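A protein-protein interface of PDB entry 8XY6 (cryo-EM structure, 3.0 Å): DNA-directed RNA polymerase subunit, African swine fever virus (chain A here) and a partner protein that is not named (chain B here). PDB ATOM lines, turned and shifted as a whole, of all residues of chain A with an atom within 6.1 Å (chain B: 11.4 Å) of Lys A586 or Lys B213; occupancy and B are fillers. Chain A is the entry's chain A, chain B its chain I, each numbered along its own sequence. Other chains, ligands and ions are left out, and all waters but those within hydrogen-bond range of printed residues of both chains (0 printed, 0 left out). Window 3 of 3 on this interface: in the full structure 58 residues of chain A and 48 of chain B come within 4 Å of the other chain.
Of the 19 printed residues of chain B, 4 touch a printed residue of chain A.
Printed residues of chain B that touch a printed residue of chain A: Arg B208, Lys B209, Ile B212 and Lys B213.
Hydrophobic or aromatic side chains of chain B within 4 Å of the printed part of chain A: Ile B212.
Of the 10 printed residues of chain A, 5 touch a printed residue of chain B.
Printed residues of chain A that touch a printed residue of chain B: Tyr A574, Glu A576, Tyr A584, Lys A586 and Ile A589.
Hydrophobic or aromatic side chains of chain A within 4 Å of the printed part of chain B: Tyr A574, Tyr A584 and Ile A589.
Among the printed residues, 7 pairs touch across the chains.
Among the printed residues, no Asp or Glu carboxylate lies within 4 Å of a Lys or Arg side-chain nitrogen of the other chain.
The side-chain hydroxyl (OH) of Tyr A574 sits close to the side-chain carboxylate (OE1) of Glu A576 (3.2 Å).
The side-chain amino group of Lys B213 sits at hydrogen-bond distance from the backbone carbonyl oxygen of Lys B209, 3.2 Å away.
Of the printed residues of chain B, Lys A586 touches Ile B212 and Lys B213.
No residue of chain B comes within 4 Å of Asn A585.
No residue of chain B comes within 4 Å of Gln A587.
No residue of chain B comes within 4 Å of Asp A588.
Printed residues of chain B within 4 Å of Tyr A574: Ile B212 (3.3 Å).
Printed residues of chain B within 4 Å of Glu A576: Arg B208 (3.2 Å) and Lys B209 (3.7 Å).
Printed residues of chain A within 4 Å of Arg B208: Glu A576 (3.2 Å).
Of the printed residues of chain A, Ile B212 touches Tyr A574 (3.3 Å), Tyr A584 (3.6 Å), Lys A586 (2.3 Å) and Ile A589 (3.6 Å).
Printed residues of chain B within 4 Å of Tyr A584: Ile B212.
Glu B205 touches none of the printed residues of chain A.
The nearest printed residue of chain B that does not touch Lys A586 is Ile B215 (5.3 Å).
The nearest residue of chain A that does not touch Lys B213 is Glu A576 (5.0 Å).
The nearest printed residue of chain B that does not touch Tyr A584 is Asn B217 (4.6 Å).
Among the printed residues, pairs that only touch across the chains: Tyr A574 with Ile B212 (3.3 Å), Ile A589 with Ile B212 (3.6 Å), Tyr A584 with Ile B212 (3.6 Å), Glu A576 with Lys B209 (3.7 Å) and Lys A586 with Lys B213 (3.9 Å).
The side-chain carboxylate (OE1) of Glu A576 sits close to the backbone carbonyl oxygen (O) of Arg B208 (3.5 Å).
The side-chain amino group of Lys A586 sits close to the backbone carbonyl oxygen of Ile B212 (2.3 Å).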
ATOM      1  N   TYR A 574     -13.179   2.650   2.265  1.00  0.00           N
ATOM      2  CA  TYR A 574     -14.395   2.026   2.764  1.00  0.00           C
ATOM      3  C   TYR A 574     -14.330   1.918   4.281  1.00  0.00           C
ATOM      4  O   TYR A 574     -13.491   1.188   4.819  1.00  0.00           O
ATOM      5  CB  TYR A 574     -14.591   0.647   2.149  1.00  0.00           C
ATOM      6  CG  TYR A 574     -15.686  -0.131   2.821  1.00  0.00           C
ATOM      7  CD1 TYR A 574     -16.981   0.352   2.853  1.00  0.00           C
ATOM      8  CD2 TYR A 574     -15.422  -1.337   3.440  1.00  0.00           C
ATOM      9  CE1 TYR A 574     -17.981  -0.346   3.470  1.00  0.00           C
ATOM     10  CE2 TYR A 574     -16.417  -2.048   4.059  1.00  0.00           C
ATOM     11  CZ  TYR A 574     -17.696  -1.548   4.072  1.00  0.00           C
ATOM     12  OH  TYR A 574     -18.696  -2.256   4.693  1.00  0.00           O
ATOM     13  N   GLU A 576     -16.963   1.517   7.819  1.00  0.00           N
ATOM     14  CA  GLU A 576     -18.323   1.259   8.276  1.00  0.00           C
ATOM     15  C   GLU A 576     -18.950   2.495   8.899  1.00  0.00           C
ATOM     16  O   GLU A 576     -20.171   2.666   8.838  1.00  0.00           O
ATOM     17  CB  GLU A 576     -18.341   0.106   9.278  1.00  0.00           C
ATOM     18  CG  GLU A 576     -17.822  -1.207   8.731  1.00  0.00           C
ATOM     19  CD  GLU A 576     -18.678  -1.756   7.609  1.00  0.00           C
ATOM     20  OE1 GLU A 576     -19.856  -1.356   7.494  1.00  0.00           O
ATOM     21  OE2 GLU A 576     -18.174  -2.599   6.838  1.00  0.00           O
ATOM     22  N   TYR A 584     -21.454   4.075  -1.232  1.00  0.00           N
ATOM     23  CA  TYR A 584     -20.216   3.494  -1.724  1.00  0.00           C
ATOM     24  C   TYR A 584     -20.474   2.720  -3.005  1.00  0.00           C
ATOM     25  O   TYR A 584     -21.419   1.932  -3.087  1.00  0.00           O
ATOM     26  CB  TYR A 584     -19.614   2.564  -0.676  1.00  0.00           C
ATOM     27  CG  TYR A 584     -18.736   3.243   0.338  1.00  0.00           C
ATOM     28  CD1 TYR A 584     -17.543   3.832  -0.039  1.00  0.00           C
ATOM     29  CD2 TYR A 584     -19.089   3.278   1.675  1.00  0.00           C
ATOM     30  CE1 TYR A 584     -16.736   4.446   0.882  1.00  0.00           C
ATOM     31  CE2 TYR A 584     -18.285   3.891   2.605  1.00  0.00           C
ATOM     32  CZ  TYR A 584     -17.109   4.476   2.203  1.00  0.00           C
ATOM     33  OH  TYR A 584     -16.298   5.090   3.125  1.00  0.00           O
ATOM     34  N   ASN A 585     -19.631   2.939  -4.006  1.00  0.00           N
ATOM     35  CA  ASN A 585     -19.676   2.107  -5.196  1.00  0.00           C
ATOM     36  C   ASN A 585     -19.185   0.710  -4.848  1.00  0.00           C
ATOM     37  O   ASN A 585     -18.081   0.545  -4.326  1.00  0.00           O
ATOM     38  CB  ASN A 585     -18.818   2.714  -6.302  1.00  0.00           C
ATOM     39  CG  ASN A 585     -19.301   2.339  -7.679  1.00  0.00           C
ATOM     40  OD1 ASN A 585     -19.811   1.241  -7.891  1.00  0.00           O
ATOM     41  ND2 ASN A 585     -19.145   3.251  -8.629  1.00  0.00           N
ATOM     42  N   LYS A 586     -20.006  -0.300  -5.140  1.00  0.00           N
ATOM     43  CA  LYS A 586     -19.655  -1.664  -4.769  1.00  0.00           C
ATOM     44  C   LYS A 586     -18.366  -2.122  -5.429  1.00  0.00           C
ATOM     45  O   LYS A 586     -17.735  -3.068  -4.947  1.00  0.00           O
ATOM     46  CB  LYS A 586     -20.794  -2.612  -5.136  1.00  0.00           C
ATOM     47  CG  LYS A 586     -22.141  -2.189  -4.586  1.00  0.00           C
ATOM     48  CD  LYS A 586     -22.286  -2.572  -3.126  1.00  0.00           C
ATOM     49  CE  LYS A 586     -22.617  -4.047  -2.973  1.00  0.00           C
ATOM     50  NZ  LYS A 586     -22.640  -4.463  -1.545  1.00  0.00           N
ATOM     51  N   GLN A 587     -17.959  -1.470  -6.514  1.00  0.00           N
ATOM     52  CA  GLN A 587     -16.716  -1.799  -7.189  1.00  0.00           C
ATOM     53  C   GLN A 587     -15.515  -1.087  -6.590  1.00  0.00           C
ATOM     54  O   GLN A 587     -14.418  -1.193  -7.146  1.00  0.00           O
ATOM     55  CB  GLN A 587     -16.817  -1.452  -8.673  1.00  0.00           C
ATOM     56  CG  GLN A 587     -17.951  -2.137  -9.390  1.00  0.00           C
ATOM     57  CD  GLN A 587     -17.944  -1.846 -10.869  1.00  0.00           C
ATOM     58  OE1 GLN A 587     -18.841  -1.183 -11.387  1.00  0.00           O
ATOM     59  NE2 GLN A 587     -16.921  -2.331 -11.561  1.00  0.00           N
ATOM     60  N   ASP A 588     -15.696  -0.349  -5.496  1.00  0.00           N
ATOM     61  CA  ASP A 588     -14.600   0.370  -4.867  1.00  0.00           C
ATOM     62  C   ASP A 588     -14.281  -0.118  -3.461  1.00  0.00           C
ATOM     63  O   ASP A 588     -13.185   0.157  -2.964  1.00  0.00           O
ATOM     64  CB  ASP A 588     -14.911   1.868  -4.815  1.00  0.00           C
ATOM     65  CG  ASP A 588     -14.824   2.524  -6.173  1.00  0.00           C
ATOM     66  OD1 ASP A 588     -14.512   1.819  -7.152  1.00  0.00           O
ATOM     67  OD2 ASP A 588     -15.060   3.747  -6.262  1.00  0.00           O
ATOM     68  N   ILE A 589     -15.203  -0.839  -2.814  1.00  0.00           N
ATOM     69  CA  ILE A 589     -15.021  -1.241  -1.423  1.00  0.00           C
ATOM     70  C   ILE A 589     -14.240  -2.537  -1.275  1.00  0.00           C
ATOM     71  O   ILE A 589     -14.044  -3.004  -0.145  1.00  0.00           O
ATOM     72  CB  ILE A 589     -16.381  -1.386  -0.714  1.00  0.00           C
ATOM     73  CG1 ILE A 589     -17.194  -2.504  -1.361  1.00  0.00           C
ATOM     74  CG2 ILE A 589     -17.137  -0.086  -0.767  1.00  0.00           C
ATOM     75  CD1 ILE A 589     -18.145  -3.187  -0.417  1.00  0.00           C
ATOM     76  N   SER A 590     -13.798  -3.142  -2.371  1.00  0.00           N
ATOM     77  CA  SER A 590     -12.964  -4.334  -2.314  1.00  0.00           C
ATOM     78  C   SER A 590     -11.869  -4.201  -3.356  1.00  0.00           C
ATOM     79  O   SER A 590     -12.160  -4.116  -4.551  1.00  0.00           O
ATOM     80  CB  SER A 590     -13.784  -5.602  -2.557  1.00  0.00           C
ATOM     81  OG  SER A 590     -12.967  -6.755  -2.464  1.00  0.00           O
ATOM     82  N   GLU A 600     -10.410  -4.342  -9.331  1.00  0.00           N
ATOM     83  CA  GLU A 600     -11.450  -4.061  -8.348  1.00  0.00           C
ATOM     84  C   GLU A 600     -11.017  -2.841  -7.551  1.00  0.00           C
ATOM     85  O   GLU A 600      -9.829  -2.508  -7.529  1.00  0.00           O
ATOM     86  CB  GLU A 600     -11.711  -5.240  -7.409  1.00  0.00           C
ATOM     87  CG  GLU A 600     -12.968  -6.030  -7.745  1.00  0.00           C
ATOM     88  CD  GLU A 600     -14.236  -5.343  -7.292  1.00  0.00           C
ATOM     89  OE1 GLU A 600     -14.147  -4.407  -6.473  1.00  0.00           O
ATOM     90  OE2 GLU A 600     -15.323  -5.737  -7.761  1.00  0.00           O
ATOM     91  N   TYR B 192     -34.045   3.505   5.570  1.00  0.00           N
ATOM     92  CA  TYR B 192     -33.807   3.962   4.211  1.00  0.00           C
ATOM     93  C   TYR B 192     -35.114   3.986   3.438  1.00  0.00           C
ATOM     94  O   TYR B 192     -35.962   3.105   3.604  1.00  0.00           O
ATOM     95  CB  TYR B 192     -32.804   3.066   3.491  1.00  0.00           C
ATOM     96  CG  TYR B 192     -31.367   3.397   3.792  1.00  0.00           C
ATOM     97  CD1 TYR B 192     -30.713   2.818   4.865  1.00  0.00           C
ATOM     98  CD2 TYR B 192     -30.666   4.292   3.001  1.00  0.00           C
ATOM     99  CE1 TYR B 192     -29.399   3.119   5.140  1.00  0.00           C
ATOM    100  CE2 TYR B 192     -29.356   4.598   3.268  1.00  0.00           C
ATOM    101  CZ  TYR B 192     -28.727   4.009   4.337  1.00  0.00           C
ATOM    102  OH  TYR B 192     -27.419   4.313   4.603  1.00  0.00           O
ATOM    103  N   GLN B 199     -39.399   1.511  -7.003  1.00  0.00           N
ATOM    104  CA  GLN B 199     -38.575   0.529  -6.303  1.00  0.00           C
ATOM    105  C   GLN B 199     -39.381  -0.002  -5.127  1.00  0.00           C
ATOM    106  O   GLN B 199     -39.533   0.667  -4.103  1.00  0.00           O
ATOM    107  CB  GLN B 199     -37.260   1.156  -5.856  1.00  0.00           C
ATOM    108  CG  GLN B 199     -36.150   0.154  -5.614  1.00  0.00           C
ATOM    109  CD  GLN B 199     -34.866   0.553  -6.308  1.00  0.00           C
ATOM    110  OE1 GLN B 199     -34.863   1.440  -7.161  1.00  0.00           O
ATOM    111  NE2 GLN B 199     -33.768  -0.103  -5.952  1.00  0.00           N
ATOM    112  N   PRO B 201     -39.233  -2.382  -2.669  1.00  0.00           N
ATOM    113  CA  PRO B 201     -38.846  -2.516  -1.256  1.00  0.00           C
ATOM    114  C   PRO B 201     -39.094  -1.255  -0.452  1.00  0.00           C
ATOM    115  O   PRO B 201     -39.444  -1.348   0.732  1.00  0.00           O
ATOM    116  CB  PRO B 201     -37.353  -2.858  -1.330  1.00  0.00           C
ATOM    117  CG  PRO B 201     -37.199  -3.539  -2.626  1.00  0.00           C
ATOM    118  CD  PRO B 201     -38.183  -2.903  -3.565  1.00  0.00           C
ATOM    119  N   ILE B 204     -36.319   0.217   3.960  1.00  0.00           N
ATOM    120  CA  ILE B 204     -35.376  -0.777   4.454  1.00  0.00           C
ATOM    121  C   ILE B 204     -34.796  -0.269   5.765  1.00  0.00           C
ATOM    122  O   ILE B 204     -34.293   0.857   5.829  1.00  0.00           O
ATOM    123  CB  ILE B 204     -34.246  -1.061   3.447  1.00  0.00           C
ATOM    124  CG1 ILE B 204     -34.801  -1.190   2.029  1.00  0.00           C
ATOM    125  CG2 ILE B 204     -33.507  -2.326   3.833  1.00  0.00           C
ATOM    126  CD1 ILE B 204     -33.781  -1.660   1.015  1.00  0.00           C
ATOM    127  N   GLU B 205     -34.869  -1.092   6.804  1.00  0.00           N
ATOM    128  CA  GLU B 205     -34.255  -0.797   8.090  1.00  0.00           C
ATOM    129  C   GLU B 205     -33.087  -1.751   8.281  1.00  0.00           C
ATOM    130  O   GLU B 205     -33.270  -2.971   8.257  1.00  0.00           O
ATOM    131  CB  GLU B 205     -35.265  -0.934   9.226  1.00  0.00           C
ATOM    132  CG  GLU B 205     -36.558  -0.189   8.975  1.00  0.00           C
ATOM    133  CD  GLU B 205     -37.390  -0.036  10.228  1.00  0.00           C
ATOM    134  OE1 GLU B 205     -37.151  -0.789  11.194  1.00  0.00           O
ATOM    135  OE2 GLU B 205     -38.283   0.836  10.248  1.00  0.00           O
ATOM    136  N   VAL B 206     -31.890  -1.197   8.469  1.00  0.00           N
ATOM    137  CA  VAL B 206     -30.664  -1.978   8.435  1.00  0.00           C
ATOM    138  C   VAL B 206     -29.755  -1.588   9.591  1.00  0.00           C
ATOM    139  O   VAL B 206     -29.925  -0.548  10.229  1.00  0.00           O
ATOM    140  CB  VAL B 206     -29.917  -1.799   7.098  1.00  0.00           C
ATOM    141  CG1 VAL B 206     -30.577  -2.624   6.020  1.00  0.00           C
ATOM    142  CG2 VAL B 206     -29.907  -0.342   6.705  1.00  0.00           C
ATOM    143  N   THR B 207     -28.790  -2.458   9.859  1.00  0.00           N
ATOM    144  CA  THR B 207     -27.690  -2.191  10.771  1.00  0.00           C
ATOM    145  C   THR B 207     -26.496  -1.677   9.966  1.00  0.00           C
ATOM    146  O   THR B 207     -26.381  -1.930   8.765  1.00  0.00           O
ATOM    147  CB  THR B 207     -27.356  -3.466  11.558  1.00  0.00           C
ATOM    148  OG1 THR B 207     -28.271  -3.598  12.653  1.00  0.00           O
ATOM    149  CG2 THR B 207     -25.934  -3.470  12.106  1.00  0.00           C
ATOM    150  N   ARG B 208     -25.622  -0.921  10.636  1.00  0.00           N
ATOM    151  CA  ARG B 208     -24.516  -0.260   9.950  1.00  0.00           C
ATOM    152  C   ARG B 208     -23.691  -1.236   9.120  1.00  0.00           C
ATOM    153  O   ARG B 208     -23.247  -0.900   8.016  1.00  0.00           O
ATOM    154  CB  ARG B 208     -23.621   0.445  10.964  1.00  0.00           C
ATOM    155  CG  ARG B 208     -22.655   1.423  10.341  1.00  0.00           C
ATOM    156  CD  ARG B 208     -22.391   2.599  11.257  1.00  0.00           C
ATOM    157  NE  ARG B 208     -21.309   2.319  12.190  1.00  0.00           N
ATOM    158  CZ  ARG B 208     -21.110   2.977  13.323  1.00  0.00           C
ATOM    159  NH1 ARG B 208     -21.919   3.949  13.707  1.00  0.00           N
ATOM    160  NH2 ARG B 208     -20.071   2.654  14.086  1.00  0.00           N
ATOM    161  N   LYS B 209     -23.458  -2.445   9.637  1.00  0.00           N
ATOM    162  CA  LYS B 209     -22.657  -3.417   8.896  1.00  0.00           C
ATOM    163  C   LYS B 209     -23.370  -3.896   7.637  1.00  0.00           C
ATOM    164  O   LYS B 209     -22.736  -4.082   6.593  1.00  0.00           O
ATOM    165  CB  LYS B 209     -22.300  -4.599   9.793  1.00  0.00           C
ATOM    166  CG  LYS B 209     -21.910  -4.207  11.201  1.00  0.00           C
ATOM    167  CD  LYS B 209     -20.472  -4.608  11.489  1.00  0.00           C
ATOM    168  CE  LYS B 209     -19.975  -4.007  12.790  1.00  0.00           C
ATOM    169  NZ  LYS B 209     -19.425  -2.639  12.589  1.00  0.00           N
ATOM    170  N   ASP B 210     -24.686  -4.098   7.710  1.00  0.00           N
ATOM    171  CA  ASP B 210     -25.423  -4.651   6.582  1.00  0.00           C
ATOM    172  C   ASP B 210     -25.770  -3.608   5.527  1.00  0.00           C
ATOM    173  O   ASP B 210     -26.333  -3.972   4.485  1.00  0.00           O
ATOM    174  CB  ASP B 210     -26.701  -5.325   7.079  1.00  0.00           C
ATOM    175  CG  ASP B 210     -26.435  -6.675   7.713  1.00  0.00           C
ATOM    176  OD1 ASP B 210     -25.540  -6.757   8.581  1.00  0.00           O
ATOM    177  OD2 ASP B 210     -27.115  -7.654   7.345  1.00  0.00           O
ATOM    178  N   VAL B 211     -25.456  -2.335   5.769  1.00  0.00           N
ATOM    179  CA  VAL B 211     -25.849  -1.276   4.843  1.00  0.00           C
ATOM    180  C   VAL B 211     -25.216  -1.502   3.477  1.00  0.00           C
ATOM    181  O   VAL B 211     -25.891  -1.439   2.443  1.00  0.00           O
ATOM    182  CB  VAL B 211     -25.473   0.101   5.415  1.00  0.00           C
ATOM    183  CG1 VAL B 211     -25.501   1.155   4.324  1.00  0.00           C
ATOM    184  CG2 VAL B 211     -26.409   0.478   6.546  1.00  0.00           C
ATOM    185  N   ILE B 212     -23.912  -1.777   3.453  1.00  0.00           N
ATOM    186  CA  ILE B 212     -23.229  -1.973   2.178  1.00  0.00           C
ATOM    187  C   ILE B 212     -23.703  -3.249   1.497  1.00  0.00           C
ATOM    188  O   ILE B 212     -23.626  -3.370   0.269  1.00  0.00           O
ATOM    189  CB  ILE B 212     -21.705  -1.965   2.384  1.00  0.00           C
ATOM    190  CG1 ILE B 212     -21.003  -1.608   1.078  1.00  0.00           C
ATOM    191  CG2 ILE B 212     -21.221  -3.304   2.906  1.00  0.00           C
ATOM    192  CD1 ILE B 212     -21.448  -0.299   0.499  1.00  0.00           C
ATOM    193  N   LYS B 213     -24.199  -4.216   2.269  1.00  0.00           N
ATOM    194  CA  LYS B 213     -24.702  -5.446   1.673  1.00  0.00           C
ATOM    195  C   LYS B 213     -26.072  -5.237   1.048  1.00  0.00           C
ATOM    196  O   LYS B 213     -26.408  -5.882   0.049  1.00  0.00           O
ATOM    197  CB  LYS B 213     -24.769  -6.555   2.723  1.00  0.00           C
ATOM    198  CG  LYS B 213     -23.437  -7.212   3.036  1.00  0.00           C
ATOM    199  CD  LYS B 213     -22.725  -6.493   4.164  1.00  0.00           C
ATOM    200  CE  LYS B 213     -21.593  -7.329   4.721  1.00  0.00           C
ATOM    201  NZ  LYS B 213     -20.968  -6.681   5.904  1.00  0.00           N
ATOM    202  N   LYS B 214     -26.880  -4.343   1.618  1.00  0.00           N
ATOM    203  CA  LYS B 214     -28.290  -4.270   1.262  1.00  0.00           C
ATOM    204  C   LYS B 214     -28.699  -3.008   0.515  1.00  0.00           C
ATOM    205  O   LYS B 214     -29.563  -3.088  -0.359  1.00  0.00           O
ATOM    206  CB  LYS B 214     -29.147  -4.403   2.523  1.00  0.00           C
ATOM    207  CG  LYS B 214     -28.945  -5.728   3.227  1.00  0.00           C
ATOM    208  CD  LYS B 214     -29.696  -5.794   4.539  1.00  0.00           C
ATOM    209  CE  LYS B 214     -29.510  -7.147   5.200  1.00  0.00           C
ATOM    210  NZ  LYS B 214     -29.969  -7.139   6.613  1.00  0.00           N
ATOM    211  N   ILE B 215     -28.116  -1.855   0.822  1.00  0.00           N
ATOM    212  CA  ILE B 215     -28.586  -0.579   0.288  1.00  0.00           C
ATOM    213  C   ILE B 215     -27.732  -0.170  -0.903  1.00  0.00           C
ATOM    214  O   ILE B 215     -26.509  -0.355  -0.904  1.00  0.00           O
ATOM    215  CB  ILE B 215     -28.578   0.514   1.374  1.00  0.00           C
ATOM    216  CG1 ILE B 215     -29.214  -0.013   2.658  1.00  0.00           C
ATOM    217  CG2 ILE B 215     -29.321   1.743   0.893  1.00  0.00           C
ATOM    218  CD1 ILE B 215     -30.648  -0.424   2.493  1.00  0.00           C
ATOM    219  N   ASP B 216     -28.382   0.397  -1.920  1.00  0.00           N
ATOM    220  CA  ASP B 216     -27.698   0.854  -3.121  1.00  0.00           C
ATOM    221  C   ASP B 216     -28.018   2.315  -3.413  1.00  0.00           C
ATOM    222  O   ASP B 216     -28.652   2.992  -2.598  1.00  0.00           O
ATOM    223  CB  ASP B 216     -28.073  -0.022  -4.317  1.00  0.00           C
ATOM    224  CG  ASP B 216     -29.572  -0.156  -4.494  1.00  0.00           C
ATOM    225  OD1 ASP B 216     -30.232   0.859  -4.793  1.00  0.00           O
ATOM    226  OD2 ASP B 216     -30.090  -1.280  -4.333  1.00  0.00           O
ATOM    227  N   ASN B 217     -27.592   2.804  -4.580  1.00  0.00           N
ATOM    228  CA  ASN B 217     -27.711   4.222  -4.897  1.00  0.00           C
ATOM    229  C   ASN B 217     -29.150   4.663  -5.124  1.00  0.00           C
ATOM    230  O   ASN B 217     -29.431   5.864  -5.059  1.00  0.00           O
ATOM    231  CB  ASN B 217     -26.867   4.544  -6.127  1.00  0.00           C
ATOM    232  CG  ASN B 217     -25.400   4.229  -5.918  1.00  0.00           C
ATOM    233  OD1 ASN B 217     -25.031   3.085  -5.655  1.00  0.00           O
ATOM    234  ND2 ASN B 217     -24.555   5.244  -6.033  1.00  0.00           N
ATOM    235  N   HIS B 218     -30.066   3.732  -5.385  1.00  0.00           N
ATOM    236  CA  HIS B 218     -31.465   4.087  -5.597  1.00  0.00           C
ATOM    237  C   HIS B 218     -32.193   4.440  -4.312  1.00  0.00           C
ATOM    238  O   HIS B 218     -33.410   4.642  -4.352  1.00  0.00           O
ATOM    239  CB  HIS B 218     -32.203   2.944  -6.293  1.00  0.00           C
ATOM    240  CG  HIS B 218     -31.771   2.720  -7.706  1.00  0.00           C
ATOM    241  ND1 HIS B 218     -31.940   3.666  -8.694  1.00  0.00           N
ATOM    242  CD2 HIS B 218     -31.180   1.657  -8.300  1.00  0.00           C
ATOM    243  CE1 HIS B 218     -31.468   3.196  -9.835  1.00  0.00           C
ATOM    244  NE2 HIS B 218     -31.002   1.979  -9.623  1.00  0.00           N
ATOM    245  N   TYR B 219     -31.500   4.509  -3.182  1.00  0.00           N
ATOM    246  CA  TYR B 219     -32.133   4.766  -1.900  1.00  0.00           C
ATOM    247  C   TYR B 219     -31.568   6.028  -1.265  1.00  0.00           C
ATOM    248  O   TYR B 219     -30.475   6.486  -1.607  1.00  0.00           O
ATOM    249  CB  TYR B 219     -31.943   3.584  -0.951  1.00  0.00           C
ATOM    250  CG  TYR B 219     -32.764   2.378  -1.321  1.00  0.00           C
ATOM    251  CD1 TYR B 219     -32.339   1.506  -2.309  1.00  0.00           C
ATOM    252  CD2 TYR B 219     -33.966   2.112  -0.683  1.00  0.00           C
ATOM    253  CE1 TYR B 219     -33.084   0.401  -2.652  1.00  0.00           C
ATOM    254  CE2 TYR B 219     -34.720   1.009  -1.019  1.00  0.00           C
ATOM    255  CZ  TYR B 219     -34.272   0.155  -2.003  1.00  0.00           C
ATOM    256  OH  TYR B 219     -35.016  -0.948  -2.348  1.00  0.00           O
